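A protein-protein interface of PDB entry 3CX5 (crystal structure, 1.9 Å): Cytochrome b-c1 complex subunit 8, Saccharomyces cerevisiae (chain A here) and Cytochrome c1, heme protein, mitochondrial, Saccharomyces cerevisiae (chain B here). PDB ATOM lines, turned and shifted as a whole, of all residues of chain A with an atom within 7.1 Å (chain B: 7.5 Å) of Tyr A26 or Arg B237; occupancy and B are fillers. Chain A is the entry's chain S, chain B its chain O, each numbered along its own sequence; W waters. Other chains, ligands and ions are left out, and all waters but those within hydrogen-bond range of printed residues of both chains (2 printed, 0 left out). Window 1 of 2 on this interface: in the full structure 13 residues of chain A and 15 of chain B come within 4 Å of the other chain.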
ATOM      1  N   THR A  24     -17.080  -7.377  24.813  1.00  0.00           N
ATOM      2  CA  THR A  24     -18.514  -7.271  25.049  1.00  0.00           C
ATOM      3  C   THR A  24     -18.747  -6.006  25.877  1.00  0.00           C
ATOM      4  O   THR A  24     -18.074  -5.793  26.883  1.00  0.00           O
ATOM      5  CB  THR A  24     -19.069  -8.489  25.815  1.00  0.00           C
ATOM      6  OG1 THR A  24     -18.832  -9.686  25.062  1.00  0.00           O
ATOM      7  CG2 THR A  24     -20.580  -8.338  26.038  1.00  0.00           C
ATOM      8  N   SER A  25     -19.648  -5.140  25.426  1.00  0.00           N
ATOM      9  CA  SER A  25     -19.945  -3.928  26.179  1.00  0.00           C
ATOM     10  C   SER A  25     -21.355  -4.011  26.736  1.00  0.00           C
ATOM     11  O   SER A  25     -22.219  -4.679  26.179  1.00  0.00           O
ATOM     12  CB  SER A  25     -19.806  -2.670  25.316  1.00  0.00           C
ATOM     13  OG  SER A  25     -20.828  -2.582  24.339  1.00  0.00           O
ATOM     14  N   TYR A  26     -21.566  -3.327  27.850  1.00  0.00           N
ATOM     15  CA  TYR A  26     -22.859  -3.289  28.514  1.00  0.00           C
ATOM     16  C   TYR A  26     -23.129  -1.843  28.899  1.00  0.00           C
ATOM     17  O   TYR A  26     -22.201  -1.097  29.231  1.00  0.00           O
ATOM     18  CB  TYR A  26     -22.825  -4.126  29.796  1.00  0.00           C
ATOM     19  CG  TYR A  26     -22.406  -5.567  29.621  1.00  0.00           C
ATOM     20  CD1 TYR A  26     -21.060  -5.919  29.564  1.00  0.00           C
ATOM     21  CD2 TYR A  26     -23.358  -6.589  29.593  1.00  0.00           C
ATOM     22  CE1 TYR A  26     -20.669  -7.255  29.492  1.00  0.00           C
ATOM     23  CE2 TYR A  26     -22.979  -7.927  29.519  1.00  0.00           C
ATOM     24  CZ  TYR A  26     -21.635  -8.250  29.473  1.00  0.00           C
ATOM     25  OH  TYR A  26     -21.254  -9.565  29.409  1.00  0.00           O
ATOM     26  N   ALA A  27     -24.396  -1.451  28.865  1.00  0.00           N
ATOM     27  CA  ALA A  27     -24.789  -0.101  29.231  1.00  0.00           C
ATOM     28  C   ALA A  27     -26.196  -0.146  29.791  1.00  0.00           C
ATOM     29  O   ALA A  27     -26.949  -1.088  29.543  1.00  0.00           O
ATOM     30  CB  ALA A  27     -24.735   0.845  28.008  1.00  0.00           C
ATOM     31  N   VAL A  28     -26.533   0.880  30.559  1.00  0.00           N
ATOM     32  CA  VAL A  28     -27.849   1.001  31.164  1.00  0.00           C
ATOM     33  C   VAL A  28     -28.434   2.347  30.769  1.00  0.00           C
ATOM     34  O   VAL A  28     -27.715   3.345  30.638  1.00  0.00           O
ATOM     35  CB  VAL A  28     -27.771   0.886  32.714  1.00  0.00           C
ATOM     36  CG1 VAL A  28     -29.126   1.200  33.336  1.00  0.00           C
ATOM     37  CG2 VAL A  28     -27.355  -0.521  33.110  1.00  0.00           C
ATOM     38  N   GLN A  33     -31.062   5.510  35.717  1.00  0.00           N
ATOM     39  CA  GLN A  33     -29.994   5.878  36.639  1.00  0.00           C
ATOM     40  C   GLN A  33     -30.388   6.991  37.599  1.00  0.00           C
ATOM     41  O   GLN A  33     -31.311   7.759  37.327  1.00  0.00           O
ATOM     42  CB  GLN A  33     -28.726   6.256  35.862  1.00  0.00           C
ATOM     43  CG  GLN A  33     -28.144   5.098  35.049  1.00  0.00           C
ATOM     44  CD  GLN A  33     -26.872   5.470  34.302  1.00  0.00           C
ATOM     45  OE1 GLN A  33     -25.965   6.096  34.859  1.00  0.00           O
ATOM     46  NE2 GLN A  33     -26.795   5.077  33.037  1.00  0.00           N
ATOM     47  N   TRP B 231     -25.462  11.870  28.502  1.00  0.00           N
ATOM     48  CA  TRP B 231     -24.209  11.123  28.463  1.00  0.00           C
ATOM     49  C   TRP B 231     -24.128   9.983  29.477  1.00  0.00           C
ATOM     50  O   TRP B 231     -23.149   9.241  29.477  1.00  0.00           O
ATOM     51  CB  TRP B 231     -23.031  12.070  28.727  1.00  0.00           C
ATOM     52  CG  TRP B 231     -22.496  12.747  27.511  1.00  0.00           C
ATOM     53  CD1 TRP B 231     -23.053  13.800  26.842  1.00  0.00           C
ATOM     54  CD2 TRP B 231     -21.269  12.438  26.831  1.00  0.00           C
ATOM     55  NE1 TRP B 231     -22.241  14.174  25.791  1.00  0.00           N
ATOM     56  CE2 TRP B 231     -21.144  13.354  25.760  1.00  0.00           C
ATOM     57  CE3 TRP B 231     -20.269  11.474  27.020  1.00  0.00           C
ATOM     58  CZ2 TRP B 231     -20.052  13.337  24.880  1.00  0.00           C
ATOM     59  CZ3 TRP B 231     -19.173  11.452  26.140  1.00  0.00           C
ATOM     60  CH2 TRP B 231     -19.079  12.382  25.085  1.00  0.00           C
ATOM     61  N   ALA B 232     -25.143   9.842  30.326  1.00  0.00           N
ATOM     62  CA  ALA B 232     -25.124   8.826  31.383  1.00  0.00           C
ATOM     63  C   ALA B 232     -24.918   7.383  30.923  1.00  0.00           C
ATOM     64  O   ALA B 232     -24.263   6.601  31.615  1.00  0.00           O
ATOM     65  CB  ALA B 232     -26.376   8.940  32.262  1.00  0.00           C
ATOM     66  N   GLY B 233     -25.467   7.040  29.762  1.00  0.00           N
ATOM     67  CA  GLY B 233     -25.316   5.695  29.240  1.00  0.00           C
ATOM     68  C   GLY B 233     -23.896   5.429  28.781  1.00  0.00           C
ATOM     69  O   GLY B 233     -23.386   4.319  28.943  1.00  0.00           O
ATOM     70  N   ILE B 234     -23.248   6.442  28.211  1.00  0.00           N
ATOM     71  CA  ILE B 234     -21.871   6.295  27.736  1.00  0.00           C
ATOM     72  C   ILE B 234     -20.879   6.323  28.899  1.00  0.00           C
ATOM     73  O   ILE B 234     -19.959   5.511  28.947  1.00  0.00           O
ATOM     74  CB  ILE B 234     -21.493   7.414  26.719  1.00  0.00           C
ATOM     75  CG1 ILE B 234     -22.323   7.273  25.438  1.00  0.00           C
ATOM     76  CG2 ILE B 234     -19.983   7.414  26.430  1.00  0.00           C
ATOM     77  CD1 ILE B 234     -22.207   5.917  24.734  1.00  0.00           C
ATOM     78  N   LYS B 235     -21.093   7.245  29.837  1.00  0.00           N
ATOM     79  CA  LYS B 235     -20.218   7.415  30.995  1.00  0.00           C
ATOM     80  C   LYS B 235     -20.075   6.177  31.870  1.00  0.00           C
ATOM     81  O   LYS B 235     -18.999   5.920  32.393  1.00  0.00           O
ATOM     82  CB  LYS B 235     -20.682   8.593  31.862  1.00  0.00           C
ATOM     83  CG  LYS B 235     -20.395   9.972  31.277  1.00  0.00           C
ATOM     84  CD  LYS B 235     -18.935  10.386  31.449  1.00  0.00           C
ATOM     85  CE  LYS B 235     -18.731  11.811  30.955  1.00  0.00           C
ATOM     86  NZ  LYS B 235     -17.465  12.422  31.434  1.00  0.00           N
ATOM     87  N   THR B 236     -21.151   5.414  32.017  1.00  0.00           N
ATOM     88  CA  THR B 236     -21.127   4.218  32.853  1.00  0.00           C
ATOM     89  C   THR B 236     -20.998   2.910  32.083  1.00  0.00           C
ATOM     90  O   THR B 236     -21.136   1.833  32.649  1.00  0.00           O
ATOM     91  CB  THR B 236     -22.356   4.167  33.758  1.00  0.00           C
ATOM     92  OG1 THR B 236     -23.539   4.245  32.957  1.00  0.00           O
ATOM     93  CG2 THR B 236     -22.329   5.338  34.744  1.00  0.00           C
ATOM     94  N   ARG B 237     -20.698   3.017  30.794  1.00  0.00           N
ATOM     95  CA  ARG B 237     -20.513   1.866  29.917  1.00  0.00           C
ATOM     96  C   ARG B 237     -19.438   0.927  30.491  1.00  0.00           C
ATOM     97  O   ARG B 237     -18.422   1.384  31.010  1.00  0.00           O
ATOM     98  CB  ARG B 237     -20.066   2.393  28.553  1.00  0.00           C
ATOM     99  CG  ARG B 237     -20.466   1.586  27.349  1.00  0.00           C
ATOM    100  CD  ARG B 237     -20.458   2.484  26.108  1.00  0.00           C
ATOM    101  NE  ARG B 237     -19.243   3.298  26.042  1.00  0.00           N
ATOM    102  CZ  ARG B 237     -18.624   3.651  24.917  1.00  0.00           C
ATOM    103  NH1 ARG B 237     -17.519   4.387  24.979  1.00  0.00           N
ATOM    104  NH2 ARG B 237     -19.107   3.282  23.734  1.00  0.00           N
ATOM    105  N   LYS B 238     -19.661  -0.382  30.388  1.00  0.00           N
ATOM    106  CA  LYS B 238     -18.704  -1.369  30.887  1.00  0.00           C
ATOM    107  C   LYS B 238     -18.260  -2.265  29.744  1.00  0.00           C
ATOM    108  O   LYS B 238     -19.086  -2.728  28.963  1.00  0.00           O
ATOM    109  CB  LYS B 238     -19.344  -2.256  31.959  1.00  0.00           C
ATOM    110  CG  LYS B 238     -20.062  -1.524  33.075  1.00  0.00           C
ATOM    111  CD  LYS B 238     -19.137  -1.157  34.206  1.00  0.00           C
ATOM    112  CE  LYS B 238     -19.946  -0.696  35.410  1.00  0.00           C
ATOM    113  NZ  LYS B 238     -19.080  -0.405  36.587  1.00  0.00           N
ATOM    114  N   PHE B 239     -16.960  -2.537  29.678  1.00  0.00           N
ATOM    115  CA  PHE B 239     -16.393  -3.395  28.647  1.00  0.00           C
ATOM    116  C   PHE B 239     -15.698  -4.608  29.281  1.00  0.00           C
ATOM    117  O   PHE B 239     -15.061  -4.486  30.328  1.00  0.00           O
ATOM    118  CB  PHE B 239     -15.364  -2.618  27.811  1.00  0.00           C
ATOM    119  CG  PHE B 239     -15.960  -1.547  26.935  1.00  0.00           C
ATOM    120  CD1 PHE B 239     -16.096  -0.236  27.398  1.00  0.00           C
ATOM    121  CD2 PHE B 239     -16.350  -1.838  25.630  1.00  0.00           C
ATOM    122  CE1 PHE B 239     -16.611   0.765  26.570  1.00  0.00           C
ATOM    123  CE2 PHE B 239     -16.864  -0.848  24.798  1.00  0.00           C
ATOM    124  CZ  PHE B 239     -16.996   0.458  25.266  1.00  0.00           C
ATOM    125  N   VAL B 240     -15.838  -5.775  28.658  1.00  0.00           N
ATOM    126  CA  VAL B 240     -15.174  -6.992  29.134  1.00  0.00           C
ATOM    127  C   VAL B 240     -14.516  -7.662  27.934  1.00  0.00           C
ATOM    128  O   VAL B 240     -15.076  -7.673  26.841  1.00  0.00           O
ATOM    129  CB  VAL B 240     -16.148  -8.013  29.807  1.00  0.00           C
ATOM    130  CG1 VAL B 240     -16.911  -7.357  30.958  1.00  0.00           C
ATOM    131  CG2 VAL B 240     -17.102  -8.609  28.791  1.00  0.00           C
ATOM    132  N   ASN B 242     -12.771 -11.195  26.393  1.00  0.00           N
ATOM    133  CA  ASN B 242     -12.586 -12.641  26.467  1.00  0.00           C
ATOM    134  C   ASN B 242     -11.837 -13.002  25.194  1.00  0.00           C
ATOM    135  O   ASN B 242     -12.432 -13.063  24.112  1.00  0.00           O
ATOM    136  CB  ASN B 242     -13.934 -13.362  26.521  1.00  0.00           C
ATOM    137  CG  ASN B 242     -14.596 -13.245  27.879  1.00  0.00           C
ATOM    138  OD1 ASN B 242     -14.105 -13.798  28.865  1.00  0.00           O
ATOM    139  ND2 ASN B 242     -15.698 -12.509  27.948  1.00  0.00           N
HETATM  140  O   HOH W   1     -24.107   2.590  30.894  1.00  0.00           O
HETATM  141  O   HOH W   2     -16.617 -10.865  25.590  1.00  0.00           O
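The backbone carbonyl oxygen (O) of Ala B232 lies within hydrogen-bond range of the side-chain amide nitrogen (NE2) of Gln A33, 3.3 Å away. The side-chain amide nitrogen (NE2) of Gln A33 lies within hydrogen-bond range of the side-chain hydroxyl (OG1) of Thr B236, 3.4 Å away. N of Tyr A26 is in hydrogen-bond range of O of Lys B238 (2.8 Å). N of Val B240 is in hydrogen-bond range of O of Thr A24, at 2.9 Å.
The side-chain hydroxyl (OG1) of Thr B236 is in hydrogen-bond range of the backbone carbonyl oxygen (O) of Ala B232, at 2.8 Å. The backbone carbonyl oxygen of Val A28 sits at hydrogen-bond distance from the side-chain amide nitrogen of Gln A33 (3.1 Å).
Among the printed residues, pairs that only touch across the chains: Thr A24 with Lys B238, Thr A24 with Phe B239, Ser A25 with Lys B238, Ser A25 with Phe B239, Tyr A26 with Arg B237, Tyr A26 with Val B240, Ala A27 with Gly B233 and Val A28 with Gly B233.
Of chain B, only Arg B237 (3.5 Å), Lys B238 (2.8 Å) and Val B240 (3.9 Å) come within 4 Å of Tyr A26. Ile B234 touches none of the printed residues of chain A. Arg B237 touches just one residue of chain A: Tyr A26. Of the printed residues of chain A, Lys B238 touches Thr A24 (3.8 Å), Ser A25 (3.2 Å) and Tyr A26 (2.8 Å). Of the printed residues of chain A, Val B240 touches Thr A24 (2.9 Å) and Tyr A26 (3.9 Å). Asn B242 touches none of the printed residues of chain A. The nearest residue of chain A that does not touch Arg B237 is Ala A27 (4.4 Å). The nearest printed residue of chain B that does not touch Gln A33 is Gly B233 (4.04 Å).
Printed residues of chain A that touch a printed residue of chain B: Thr A24, Ser A25, Tyr A26, Ala A27, Val A28 and Gln A33. Hydrophobic or aromatic side chains of chain A within 4 Å of the printed part of chain B: Tyr A26 and Ala A27. Hydrophobic or aromatic side chains of chain B within 4 Å of the printed part of chain A: Ala B232, Phe B239 and Val B240. Among the printed residues, no Asp or Glu carboxylate lies within 4 Å of a Lys or Arg side-chain nitrogen of the other chain.
Water W2 lies within hydrogen-bond range of OG1 of Thr A24 (2.6 Å) and ND2 of Asn B242 (3.0 Å). Water W1 lies within hydrogen-bond range of the side-chain hydroxyl of Thr B236, the backbone carbonyl oxygen of Gly B233, the backbone NH of Val A28 and the backbone NH of Arg B237.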
